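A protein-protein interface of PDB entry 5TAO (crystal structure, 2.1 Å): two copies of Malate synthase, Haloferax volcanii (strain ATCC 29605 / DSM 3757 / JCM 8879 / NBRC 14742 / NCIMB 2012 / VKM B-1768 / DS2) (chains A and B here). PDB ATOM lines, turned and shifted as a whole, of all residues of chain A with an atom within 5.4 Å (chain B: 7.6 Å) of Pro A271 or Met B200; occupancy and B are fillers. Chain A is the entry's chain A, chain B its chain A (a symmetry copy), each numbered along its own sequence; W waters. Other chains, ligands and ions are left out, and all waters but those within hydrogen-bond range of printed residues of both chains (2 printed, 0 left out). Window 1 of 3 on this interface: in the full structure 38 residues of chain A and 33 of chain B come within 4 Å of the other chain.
The backbone carbonyl oxygen (O) of Gln A249 is in hydrogen-bond range of the backbone NH (N) of Met B200 (2.8 Å).
The backbone NH (N) of Ala A250 is in hydrogen-bond range of the backbone carbonyl oxygen (O) of Met B200 (3.4 Å).
O of Pro A273 lies within hydrogen-bond range of NH2 of Arg B419 (3.2 Å).
The backbone carbonyl oxygen (O) of Pro A273 lies within hydrogen-bond range of the side-chain hydroxyl (OH) of Tyr B420.
O of Met B197 lies close to O of Gly A252 (3.5 Å).
The backbone carbonyl oxygen of Asn A268 sits at hydrogen-bond distance from the guanidinium group of Arg A12 (3.0 Å).
The side-chain hydroxyl (OG) of Ser A270 is in hydrogen-bond range of the side-chain amide nitrogen (NE2) of Gln A249, 3.0 Å away.
The backbone carbonyl oxygen (O) of Thr B194 lies within hydrogen-bond range of the backbone NH (N) of Ala B199 (2.9 Å).
OG1 of Thr B194 is in hydrogen-bond range of NE1 of Trp B209 (3.1 Å).
The side-chain hydroxyl of Tyr B420 is in hydrogen-bond range of the guanidinium group of Arg B419.
Among the printed residues, merely in contact across the chains: Arg A12 with Val B405 (3.3 Å), Gln A249 with Ala B199 (3.3 Å), Ala A250 with Ala B199 (3.6 Å), Ala A250 with Pro B207 (3.2 Å), Ala A250 with Trp B209 (3.6 Å), Gly A252 with Arg B198 (3.5 Å), Gly A252 with Ala B199 (3.5 Å), Leu A254 with Arg B198 (3.6 Å), Thr A269 with Arg B419 (3.3 Å), Pro A271 with Met B200 (3.4 Å), Pro A271 with Leu B401 (3.6 Å) and Leu A272 with Tyr B420 (3.3 Å).
Thr A246 touches none of the printed residues of chain B.
Printed residues of chain B within 4 Å of Leu A254: Arg B198.
Of the printed residues of chain B, Pro A273 touches Arg B419 (3.2 Å) and Tyr B420 (2.6 Å).
Printed residues of chain A within 4 Å of Arg B198: Gly A252 (3.5 Å) and Leu A254 (3.6 Å).
Printed residues of chain A within 4 Å of Ala B199: Gln A249, Ala A250 and Gly A252.
Glu B205 touches none of the printed residues of chain A.
The nearest residue of chain B that does not touch Pro A271 is Pro B398 (4.3 Å).
Printed residues of chain A that touch a printed residue of chain B: Arg A12, Gln A249, Ala A250, Gly A252, Leu A254, Thr A269, Pro A271, Leu A272 and Pro A273.
Hydrophobic or aromatic side chains of chain A that line the printed part of chain B: Leu A254, Pro A271, Leu A272 and Pro A273.
Among the printed residues, 17 pairs touch across the chains.
Among the printed residues, no Asp or Glu carboxylate lies within 4 Å of a Lys or Arg side-chain nitrogen of the other chain.
No position is printed for both chains.
Water W1 lies within hydrogen-bond range of O of Met B200 (2.6 Å), O of Thr A246 (2.8 Å) and N of Ala A250 (3.4 Å).
Water W2 bridges the backbone carbonyl oxygen of Gly A252 (2.8 Å) and the guanidinium group of Arg B198 (3.0 Å).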
ATOM      1  N   ARG A  12      10.290  23.985   1.574  1.00  0.00           N
ATOM      2  CA  ARG A  12      11.338  22.986   1.458  1.00  0.00           C
ATOM      3  C   ARG A  12      12.217  22.940   2.616  1.00  0.00           C
ATOM      4  O   ARG A  12      12.687  21.868   2.974  1.00  0.00           O
ATOM      5  CB  ARG A  12      12.202  23.221   0.197  1.00  0.00           C
ATOM      6  CG  ARG A  12      11.470  23.085  -1.101  1.00  0.00           C
ATOM      7  CD  ARG A  12      12.270  23.687  -2.282  1.00  0.00           C
ATOM      8  NE  ARG A  12      12.372  25.111  -2.144  1.00  0.00           N
ATOM      9  CZ  ARG A  12      13.220  25.910  -2.820  1.00  0.00           C
ATOM     10  NH1 ARG A  12      14.048  25.431  -3.743  1.00  0.00           N
ATOM     11  NH2 ARG A  12      13.233  27.199  -2.571  1.00  0.00           N
ATOM     12  N   THR A 246      14.462  11.956   0.790  1.00  0.00           N
ATOM     13  CA  THR A 246      13.776  11.036  -0.140  1.00  0.00           C
ATOM     14  C   THR A 246      12.713  10.160   0.535  1.00  0.00           C
ATOM     15  O   THR A 246      11.624   9.964  -0.022  1.00  0.00           O
ATOM     16  CB  THR A 246      14.832  10.127  -0.832  1.00  0.00           C
ATOM     17  OG1 THR A 246      15.754  10.965  -1.543  1.00  0.00           O
ATOM     18  CG2 THR A 246      14.200   9.116  -1.782  1.00  0.00           C
ATOM     19  N   GLN A 249       9.785  12.367   1.296  1.00  0.00           N
ATOM     20  CA  GLN A 249       9.051  12.752   0.104  1.00  0.00           C
ATOM     21  C   GLN A 249       8.097  11.646  -0.310  1.00  0.00           C
ATOM     22  O   GLN A 249       7.017  11.892  -0.837  1.00  0.00           O
ATOM     23  CB  GLN A 249      10.019  13.124  -1.028  1.00  0.00           C
ATOM     24  CG  GLN A 249      10.829  14.353  -0.676  1.00  0.00           C
ATOM     25  CD  GLN A 249      12.109  14.517  -1.497  1.00  0.00           C
ATOM     26  OE1 GLN A 249      12.396  13.764  -2.419  1.00  0.00           O
ATOM     27  NE2 GLN A 249      12.862  15.495  -1.143  1.00  0.00           N
ATOM     28  N   ALA A 250       8.484  10.442  -0.033  1.00  0.00           N
ATOM     29  CA  ALA A 250       7.620   9.294  -0.278  1.00  0.00           C
ATOM     30  C   ALA A 250       6.443   9.225   0.718  1.00  0.00           C
ATOM     31  O   ALA A 250       5.520   8.472   0.459  1.00  0.00           O
ATOM     32  CB  ALA A 250       8.437   7.993  -0.294  1.00  0.00           C
ATOM     33  N   GLY A 252       4.947  12.179   1.648  1.00  0.00           N
ATOM     34  CA  GLY A 252       4.362  13.471   1.380  1.00  0.00           C
ATOM     35  C   GLY A 252       4.790  14.549   2.365  1.00  0.00           C
ATOM     36  O   GLY A 252       4.074  15.548   2.576  1.00  0.00           O
ATOM     37  N   LEU A 254       7.483  17.067   2.419  1.00  0.00           N
ATOM     38  CA  LEU A 254       8.372  17.595   1.407  1.00  0.00           C
ATOM     39  C   LEU A 254       9.253  18.680   1.936  1.00  0.00           C
ATOM     40  O   LEU A 254      10.057  19.209   1.195  1.00  0.00           O
ATOM     41  CB  LEU A 254       7.575  18.121   0.234  1.00  0.00           C
ATOM     42  CG  LEU A 254       6.577  17.163  -0.430  1.00  0.00           C
ATOM     43  CD1 LEU A 254       5.977  17.860  -1.648  1.00  0.00           C
ATOM     44  CD2 LEU A 254       7.129  15.817  -0.852  1.00  0.00           C
ATOM     45  N   GLU A 266      21.175  21.804   0.184  1.00  0.00           N
ATOM     46  CA  GLU A 266      20.783  20.400  -0.070  1.00  0.00           C
ATOM     47  C   GLU A 266      19.277  20.167  -0.030  1.00  0.00           C
ATOM     48  O   GLU A 266      18.679  19.483  -0.908  1.00  0.00           O
ATOM     49  CB  GLU A 266      21.430  19.496   0.972  1.00  0.00           C
ATOM     50  CG  GLU A 266      22.915  19.249   0.709  1.00  0.00           C
ATOM     51  CD  GLU A 266      23.101  18.193  -0.380  1.00  0.00           C
ATOM     52  OE1 GLU A 266      22.753  17.019  -0.134  1.00  0.00           O
ATOM     53  OE2 GLU A 266      23.551  18.546  -1.487  1.00  0.00           O
ATOM     54  N   ALA A 267      18.648  20.770   0.967  1.00  0.00           N
ATOM     55  CA  ALA A 267      17.185  20.595   1.143  1.00  0.00           C
ATOM     56  C   ALA A 267      16.425  21.408   0.136  1.00  0.00           C
ATOM     57  O   ALA A 267      15.336  21.009  -0.307  1.00  0.00           O
ATOM     58  CB  ALA A 267      16.788  20.920   2.574  1.00  0.00           C
ATOM     59  N   ASN A 268      17.012  22.514  -0.335  1.00  0.00           N
ATOM     60  CA  ASN A 268      16.325  23.323  -1.352  1.00  0.00           C
ATOM     61  C   ASN A 268      16.354  22.626  -2.693  1.00  0.00           C
ATOM     62  O   ASN A 268      15.452  22.776  -3.557  1.00  0.00           O
ATOM     63  CB  ASN A 268      16.921  24.730  -1.427  1.00  0.00           C
ATOM     64  CG  ASN A 268      16.284  25.688  -0.471  1.00  0.00           C
ATOM     65  OD1 ASN A 268      15.212  25.443   0.048  1.00  0.00           O
ATOM     66  ND2 ASN A 268      16.895  26.821  -0.291  1.00  0.00           N
ATOM     67  N   THR A 269      17.344  21.764  -2.851  1.00  0.00           N
ATOM     68  CA  THR A 269      17.568  21.115  -4.148  1.00  0.00           C
ATOM     69  C   THR A 269      16.916  19.741  -4.212  1.00  0.00           C
ATOM     70  O   THR A 269      16.464  19.342  -5.263  1.00  0.00           O
ATOM     71  CB  THR A 269      19.094  20.893  -4.351  1.00  0.00           C
ATOM     72  OG1 THR A 269      19.794  22.125  -4.140  1.00  0.00           O
ATOM     73  CG2 THR A 269      19.352  20.336  -5.681  1.00  0.00           C
ATOM     74  N   SER A 270      16.874  19.021  -3.085  1.00  0.00           N
ATOM     75  CA  SER A 270      16.406  17.645  -3.074  1.00  0.00           C
ATOM     76  C   SER A 270      15.048  17.365  -3.703  1.00  0.00           C
ATOM     77  O   SER A 270      14.925  16.374  -4.389  1.00  0.00           O
ATOM     78  CB  SER A 270      16.389  17.072  -1.658  1.00  0.00           C
ATOM     79  OG  SER A 270      15.760  15.793  -1.714  1.00  0.00           O
ATOM     80  N   PRO A 271      13.995  18.179  -3.421  1.00  0.00           N
ATOM     81  CA  PRO A 271      12.679  17.810  -3.986  1.00  0.00           C
ATOM     82  C   PRO A 271      12.373  18.272  -5.454  1.00  0.00           C
ATOM     83  O   PRO A 271      11.319  17.934  -6.069  1.00  0.00           O
ATOM     84  CB  PRO A 271      11.712  18.441  -3.013  1.00  0.00           C
ATOM     85  CG  PRO A 271      12.454  19.562  -2.400  1.00  0.00           C
ATOM     86  CD  PRO A 271      13.854  19.059  -2.265  1.00  0.00           C
ATOM     87  N   LEU A 272      13.296  19.043  -5.981  1.00  0.00           N
ATOM     88  CA  LEU A 272      13.298  19.421  -7.392  1.00  0.00           C
ATOM     89  C   LEU A 272      13.731  18.260  -8.306  1.00  0.00           C
ATOM     90  O   LEU A 272      14.671  17.479  -7.981  1.00  0.00           O
ATOM     91  CB  LEU A 272      14.234  20.609  -7.587  1.00  0.00           C
ATOM     92  CG  LEU A 272      13.993  21.800  -6.680  1.00  0.00           C
ATOM     93  CD1 LEU A 272      15.032  22.891  -6.898  1.00  0.00           C
ATOM     94  CD2 LEU A 272      12.562  22.287  -6.870  1.00  0.00           C
ATOM     95  N   PRO A 273      13.104  18.161  -9.476  1.00  0.00           N
ATOM     96  CA  PRO A 273      13.456  17.052 -10.383  1.00  0.00           C
ATOM     97  C   PRO A 273      14.945  17.103 -10.813  1.00  0.00           C
ATOM     98  O   PRO A 273      15.551  18.177 -10.812  1.00  0.00           O
ATOM     99  CB  PRO A 273      12.494  17.229 -11.544  1.00  0.00           C
ATOM    100  CG  PRO A 273      11.419  18.144 -11.023  1.00  0.00           C
ATOM    101  CD  PRO A 273      12.090  19.056 -10.065  1.00  0.00           C
ATOM    102  N   THR B 194      -1.691   8.718  -2.692  1.00  0.00           N
ATOM    103  CA  THR B 194      -0.403   9.348  -2.977  1.00  0.00           C
ATOM    104  C   THR B 194      -0.432  10.805  -3.400  1.00  0.00           C
ATOM    105  O   THR B 194       0.339  11.691  -2.905  1.00  0.00           O
ATOM    106  CB  THR B 194       0.384   8.542  -4.030  1.00  0.00           C
ATOM    107  OG1 THR B 194       0.516   7.225  -3.606  1.00  0.00           O
ATOM    108  CG2 THR B 194       1.770   9.092  -4.284  1.00  0.00           C
ATOM    109  N   LYS B 195      -1.377  11.113  -4.229  1.00  0.00           N
ATOM    110  CA  LYS B 195      -1.527  12.493  -4.657  1.00  0.00           C
ATOM    111  C   LYS B 195      -2.163  13.310  -3.558  1.00  0.00           C
ATOM    112  O   LYS B 195      -1.732  14.409  -3.283  1.00  0.00           O
ATOM    113  CB  LYS B 195      -2.426  12.493  -5.906  1.00  0.00           C
ATOM    114  CG  LYS B 195      -2.782  13.831  -6.493  1.00  0.00           C
ATOM    115  CD  LYS B 195      -1.561  14.673  -6.727  1.00  0.00           C
ATOM    116  CE  LYS B 195      -1.940  15.946  -7.545  1.00  0.00           C
ATOM    117  NZ  LYS B 195      -0.721  16.666  -7.957  1.00  0.00           N
ATOM    118  N   MET B 197      -1.783  12.984  -0.449  1.00  0.00           N
ATOM    119  CA  MET B 197      -0.739  13.168   0.517  1.00  0.00           C
ATOM    120  C   MET B 197       0.437  14.021  -0.010  1.00  0.00           C
ATOM    121  O   MET B 197       1.299  14.408   0.774  1.00  0.00           O
ATOM    122  CB  MET B 197      -0.218  11.823   0.980  1.00  0.00           C
ATOM    123  CG  MET B 197      -1.270  11.066   1.783  1.00  0.00           C
ATOM    124  SD  MET B 197      -1.497  11.671   3.472  1.00  0.00           S
ATOM    125  CE  MET B 197      -0.197  10.712   4.206  1.00  0.00           C
ATOM    126  N   ARG B 198       0.444  14.270  -1.311  1.00  0.00           N
ATOM    127  CA  ARG B 198       1.459  15.030  -2.054  1.00  0.00           C
ATOM    128  C   ARG B 198       2.774  14.359  -1.962  1.00  0.00           C
ATOM    129  O   ARG B 198       3.768  14.997  -1.756  1.00  0.00           O
ATOM    130  CB  ARG B 198       1.629  16.481  -1.576  1.00  0.00           C
ATOM    131  CG  ARG B 198       0.402  17.334  -1.558  1.00  0.00           C
ATOM    132  CD  ARG B 198       0.757  18.819  -1.690  1.00  0.00           C
ATOM    133  NE  ARG B 198       1.528  19.333  -0.569  1.00  0.00           N
ATOM    134  CZ  ARG B 198       1.772  20.625  -0.343  1.00  0.00           C
ATOM    135  NH1 ARG B 198       1.248  21.570  -1.121  1.00  0.00           N
ATOM    136  NH2 ARG B 198       2.524  20.973   0.687  1.00  0.00           N
ATOM    137  N   ALA B 199       2.772  13.053  -2.003  1.00  0.00           N
ATOM    138  CA  ALA B 199       3.987  12.324  -1.932  1.00  0.00           C
ATOM    139  C   ALA B 199       4.626  12.205  -3.339  1.00  0.00           C
ATOM    140  O   ALA B 199       3.988  12.453  -4.379  1.00  0.00           O
ATOM    141  CB  ALA B 199       3.712  10.950  -1.424  1.00  0.00           C
ATOM    142  N   MET B 200       5.866  11.792  -3.361  1.00  0.00           N
ATOM    143  CA  MET B 200       6.548  11.595  -4.642  1.00  0.00           C
ATOM    144  C   MET B 200       7.723  10.662  -4.471  1.00  0.00           C
ATOM    145  O   MET B 200       8.293  10.587  -3.384  1.00  0.00           O
ATOM    146  CB  MET B 200       6.959  12.929  -5.262  1.00  0.00           C
ATOM    147  CG  MET B 200       8.088  13.668  -4.648  1.00  0.00           C
ATOM    148  SD  MET B 200       8.223  15.350  -5.310  1.00  0.00           S
ATOM    149  CE  MET B 200       9.515  15.789  -4.216  1.00  0.00           C
ATOM    150  N   THR B 201       8.003   9.886  -5.525  1.00  0.00           N
ATOM    151  CA  THR B 201       9.161   9.001  -5.573  1.00  0.00           C
ATOM    152  C   THR B 201      10.022   9.318  -6.851  1.00  0.00           C
ATOM    153  O   THR B 201       9.512   9.795  -7.865  1.00  0.00           O
ATOM    154  CB  THR B 201       8.744   7.545  -5.618  1.00  0.00           C
ATOM    155  OG1 THR B 201       8.002   7.333  -6.831  1.00  0.00           O
ATOM    156  CG2 THR B 201       7.825   7.188  -4.373  1.00  0.00           C
ATOM    157  N   PRO B 202      11.309   9.034  -6.803  1.00  0.00           N
ATOM    158  CA  PRO B 202      12.176   9.265  -7.984  1.00  0.00           C
ATOM    159  C   PRO B 202      11.648   8.572  -9.251  1.00  0.00           C
ATOM    160  O   PRO B 202      11.461   9.233 -10.260  1.00  0.00           O
ATOM    161  CB  PRO B 202      13.525   8.715  -7.531  1.00  0.00           C
ATOM    162  CG  PRO B 202      13.506   8.902  -6.047  1.00  0.00           C
ATOM    163  CD  PRO B 202      12.079   8.572  -5.656  1.00  0.00           C
ATOM    164  N   THR B 203      11.260   7.308  -9.168  1.00  0.00           N
ATOM    165  CA  THR B 203      10.727   6.641 -10.364  1.00  0.00           C
ATOM    166  C   THR B 203       9.285   6.924 -10.682  1.00  0.00           C
ATOM    167  O   THR B 203       8.873   6.705 -11.795  1.00  0.00           O
ATOM    168  CB  THR B 203      10.888   5.118 -10.312  1.00  0.00           C
ATOM    169  OG1 THR B 203      10.096   4.535  -9.254  1.00  0.00           O
ATOM    170  CG2 THR B 203      12.354   4.769 -10.080  1.00  0.00           C
ATOM    171  N   GLY B 204       8.468   7.356  -9.719  1.00  0.00           N
ATOM    172  CA  GLY B 204       7.045   7.405  -9.997  1.00  0.00           C
ATOM    173  C   GLY B 204       6.337   6.169  -9.527  1.00  0.00           C
ATOM    174  O   GLY B 204       5.138   6.175  -9.535  1.00  0.00           O
ATOM    175  N   GLU B 205       7.067   5.120  -9.107  1.00  0.00           N
ATOM    176  CA  GLU B 205       6.496   3.985  -8.390  1.00  0.00           C
ATOM    177  C   GLU B 205       5.720   4.528  -7.174  1.00  0.00           C
ATOM    178  O   GLU B 205       6.111   5.539  -6.580  1.00  0.00           O
ATOM    179  CB  GLU B 205       7.569   3.019  -7.853  1.00  0.00           C
ATOM    180  CG  GLU B 205       7.033   1.594  -7.605  1.00  0.00           C
ATOM    181  CD  GLU B 205       7.939   0.640  -6.761  1.00  0.00           C
ATOM    182  OE1 GLU B 205       7.427  -0.377  -6.215  1.00  0.00           O
ATOM    183  OE2 GLU B 205       9.147   0.887  -6.637  1.00  0.00           O
ATOM    184  N   LEU B 206       4.633   3.850  -6.817  1.00  0.00           N
ATOM    185  CA  LEU B 206       3.855   4.231  -5.643  1.00  0.00           C
ATOM    186  C   LEU B 206       4.606   3.906  -4.351  1.00  0.00           C
ATOM    187  O   LEU B 206       5.194   2.861  -4.255  1.00  0.00           O
ATOM    188  CB  LEU B 206       2.507   3.479  -5.654  1.00  0.00           C
ATOM    189  CG  LEU B 206       1.488   3.815  -6.725  1.00  0.00           C
ATOM    190  CD1 LEU B 206       0.232   3.031  -6.380  1.00  0.00           C
ATOM    191  CD2 LEU B 206       1.227   5.305  -6.807  1.00  0.00           C
ATOM    192  N   PRO B 207       4.624   4.818  -3.356  1.00  0.00           N
ATOM    193  CA  PRO B 207       5.071   4.336  -2.068  1.00  0.00           C
ATOM    194  C   PRO B 207       4.243   3.123  -1.623  1.00  0.00           C
ATOM    195  O   PRO B 207       3.113   2.908  -2.061  1.00  0.00           O
ATOM    196  CB  PRO B 207       4.810   5.531  -1.115  1.00  0.00           C
ATOM    197  CG  PRO B 207       4.527   6.711  -2.012  1.00  0.00           C
ATOM    198  CD  PRO B 207       4.006   6.153  -3.292  1.00  0.00           C
ATOM    199  N   TRP B 209       3.205   2.561   1.535  1.00  0.00           N
ATOM    200  CA  TRP B 209       2.229   3.078   2.496  1.00  0.00           C
ATOM    201  C   TRP B 209       1.794   1.975   3.457  1.00  0.00           C
ATOM    202  O   TRP B 209       0.615   1.701   3.587  1.00  0.00           O
ATOM    203  CB  TRP B 209       1.024   3.574   1.750  1.00  0.00           C
ATOM    204  CG  TRP B 209       1.220   4.766   0.931  1.00  0.00           C
ATOM    205  CD1 TRP B 209       0.975   4.882  -0.384  1.00  0.00           C
ATOM    206  CD2 TRP B 209       1.560   6.069   1.394  1.00  0.00           C
ATOM    207  NE1 TRP B 209       1.153   6.165  -0.803  1.00  0.00           N
ATOM    208  CE2 TRP B 209       1.475   6.937   0.283  1.00  0.00           C
ATOM    209  CE3 TRP B 209       1.892   6.592   2.654  1.00  0.00           C
ATOM    210  CZ2 TRP B 209       1.767   8.299   0.360  1.00  0.00           C
ATOM    211  CZ3 TRP B 209       2.147   7.964   2.738  1.00  0.00           C
ATOM    212  CH2 TRP B 209       2.084   8.788   1.608  1.00  0.00           C
ATOM    213  N   ALA B 394       0.567  12.773 -10.818  1.00  0.00           N
ATOM    214  CA  ALA B 394       1.767  12.487 -10.067  1.00  0.00           C
ATOM    215  C   ALA B 394       2.893  13.454 -10.475  1.00  0.00           C
ATOM    216  O   ALA B 394       3.595  14.026  -9.623  1.00  0.00           O
ATOM    217  CB  ALA B 394       2.194  11.053 -10.265  1.00  0.00           C
ATOM    218  N   ALA B 395       3.043  13.694 -11.771  1.00  0.00           N
ATOM    219  CA  ALA B 395       4.094  14.614 -12.205  1.00  0.00           C
ATOM    220  C   ALA B 395       3.810  16.009 -11.699  1.00  0.00           C
ATOM    221  O   ALA B 395       4.749  16.756 -11.415  1.00  0.00           O
ATOM    222  CB  ALA B 395       4.255  14.623 -13.730  1.00  0.00           C
ATOM    223  N   THR B 397       2.889  17.035  -9.012  1.00  0.00           N
ATOM    224  CA  THR B 397       3.466  17.347  -7.691  1.00  0.00           C
ATOM    225  C   THR B 397       4.824  18.059  -7.746  1.00  0.00           C
ATOM    226  O   THR B 397       4.928  19.213  -7.323  1.00  0.00           O
ATOM    227  CB  THR B 397       3.462  16.143  -6.714  1.00  0.00           C
ATOM    228  OG1 THR B 397       2.102  15.742  -6.465  1.00  0.00           O
ATOM    229  CG2 THR B 397       4.108  16.550  -5.468  1.00  0.00           C
ATOM    230  N   PRO B 398       5.869  17.391  -8.229  1.00  0.00           N
ATOM    231  CA  PRO B 398       7.162  18.138  -8.299  1.00  0.00           C
ATOM    232  C   PRO B 398       7.133  19.410  -9.161  1.00  0.00           C
ATOM    233  O   PRO B 398       7.810  20.396  -8.865  1.00  0.00           O
ATOM    234  CB  PRO B 398       8.129  17.146  -8.915  1.00  0.00           C
ATOM    235  CG  PRO B 398       7.396  15.895  -9.195  1.00  0.00           C
ATOM    236  CD  PRO B 398       5.990  15.978  -8.615  1.00  0.00           C
ATOM    237  N   ILE B 399       6.356  19.386 -10.221  1.00  0.00           N
ATOM    238  CA  ILE B 399       6.242  20.586 -11.054  1.00  0.00           C
ATOM    239  C   ILE B 399       5.521  21.693 -10.292  1.00  0.00           C
ATOM    240  O   ILE B 399       5.978  22.825 -10.321  1.00  0.00           O
ATOM    241  CB  ILE B 399       5.454  20.312 -12.341  1.00  0.00           C
ATOM    242  CG1 ILE B 399       6.130  19.264 -13.206  1.00  0.00           C
ATOM    243  CG2 ILE B 399       5.212  21.610 -13.095  1.00  0.00           C
ATOM    244  CD1 ILE B 399       7.614  19.470 -13.424  1.00  0.00           C
ATOM    245  N   LEU B 401       5.484  22.137  -7.216  1.00  0.00           N
ATOM    246  CA  LEU B 401       6.465  22.542  -6.268  1.00  0.00           C
ATOM    247  C   LEU B 401       7.496  23.436  -6.963  1.00  0.00           C
ATOM    248  O   LEU B 401       7.906  24.463  -6.419  1.00  0.00           O
ATOM    249  CB  LEU B 401       7.170  21.333  -5.708  1.00  0.00           C
ATOM    250  CG  LEU B 401       8.480  21.582  -4.963  1.00  0.00           C
ATOM    251  CD1 LEU B 401       8.370  22.676  -3.959  1.00  0.00           C
ATOM    252  CD2 LEU B 401       8.855  20.314  -4.226  1.00  0.00           C
ATOM    253  N   PHE B 402       7.993  23.009  -8.109  1.00  0.00           N
ATOM    254  CA  PHE B 402       8.965  23.876  -8.837  1.00  0.00           C
ATOM    255  C   PHE B 402       8.363  25.277  -9.076  1.00  0.00           C
ATOM    256  O   PHE B 402       9.009  26.271  -8.856  1.00  0.00           O
ATOM    257  CB  PHE B 402       9.412  23.275 -10.170  1.00  0.00           C
ATOM    258  CG  PHE B 402      10.269  24.207 -10.944  1.00  0.00           C
ATOM    259  CD1 PHE B 402      11.608  24.354 -10.623  1.00  0.00           C
ATOM    260  CD2 PHE B 402       9.710  25.038 -11.893  1.00  0.00           C
ATOM    261  CE1 PHE B 402      12.389  25.253 -11.302  1.00  0.00           C
ATOM    262  CE2 PHE B 402      10.483  25.961 -12.559  1.00  0.00           C
ATOM    263  CZ  PHE B 402      11.807  26.072 -12.263  1.00  0.00           C
ATOM    264  N   VAL B 405       8.074  27.484  -6.027  1.00  0.00           N
ATOM    265  CA  VAL B 405       9.380  28.001  -5.721  1.00  0.00           C
ATOM    266  C   VAL B 405       9.676  29.198  -6.638  1.00  0.00           C
ATOM    267  O   VAL B 405      10.064  30.282  -6.156  1.00  0.00           O
ATOM    268  CB  VAL B 405      10.454  26.913  -5.845  1.00  0.00           C
ATOM    269  CG1 VAL B 405      11.827  27.512  -5.897  1.00  0.00           C
ATOM    270  CG2 VAL B 405      10.383  25.914  -4.681  1.00  0.00           C
ATOM    271  N   ARG B 419      20.584  25.710 -13.429  1.00  0.00           N
ATOM    272  CA  ARG B 419      20.365  24.288 -13.107  1.00  0.00           C
ATOM    273  C   ARG B 419      19.729  23.526 -14.267  1.00  0.00           C
ATOM    274  O   ARG B 419      20.139  22.414 -14.565  1.00  0.00           O
ATOM    275  CB  ARG B 419      19.499  24.117 -11.813  1.00  0.00           C
ATOM    276  CG  ARG B 419      19.208  22.668 -11.415  1.00  0.00           C
ATOM    277  CD  ARG B 419      18.493  22.579 -10.039  1.00  0.00           C
ATOM    278  NE  ARG B 419      17.984  21.227  -9.841  1.00  0.00           N
ATOM    279  CZ  ARG B 419      18.700  20.229  -9.336  1.00  0.00           C
ATOM    280  NH1 ARG B 419      19.934  20.449  -8.901  1.00  0.00           N
ATOM    281  NH2 ARG B 419      18.155  19.015  -9.228  1.00  0.00           N
ATOM    282  N   TYR B 420      18.706  24.104 -14.882  1.00  0.00           N
ATOM    283  CA  TYR B 420      17.933  23.445 -15.925  1.00  0.00           C
ATOM    284  C   TYR B 420      18.095  24.065 -17.329  1.00  0.00           C
ATOM    285  O   TYR B 420      17.564  23.503 -18.290  1.00  0.00           O
ATOM    286  CB  TYR B 420      16.428  23.519 -15.562  1.00  0.00           C
ATOM    287  CG  TYR B 420      16.085  22.824 -14.250  1.00  0.00           C
ATOM    288  CD1 TYR B 420      16.200  21.436 -14.137  1.00  0.00           C
ATOM    289  CD2 TYR B 420      15.685  23.537 -13.128  1.00  0.00           C
ATOM    290  CE1 TYR B 420      15.925  20.773 -12.955  1.00  0.00           C
ATOM    291  CE2 TYR B 420      15.406  22.879 -11.922  1.00  0.00           C
ATOM    292  CZ  TYR B 420      15.511  21.498 -11.853  1.00  0.00           C
ATOM    293  OH  TYR B 420      15.237  20.806 -10.706  1.00  0.00           O
HETATM  294  O   HOH W   1      10.642   9.720  -2.616  1.00  0.00           O
HETATM  295  O   HOH W   2       3.549  17.486   0.659  1.00  0.00           O
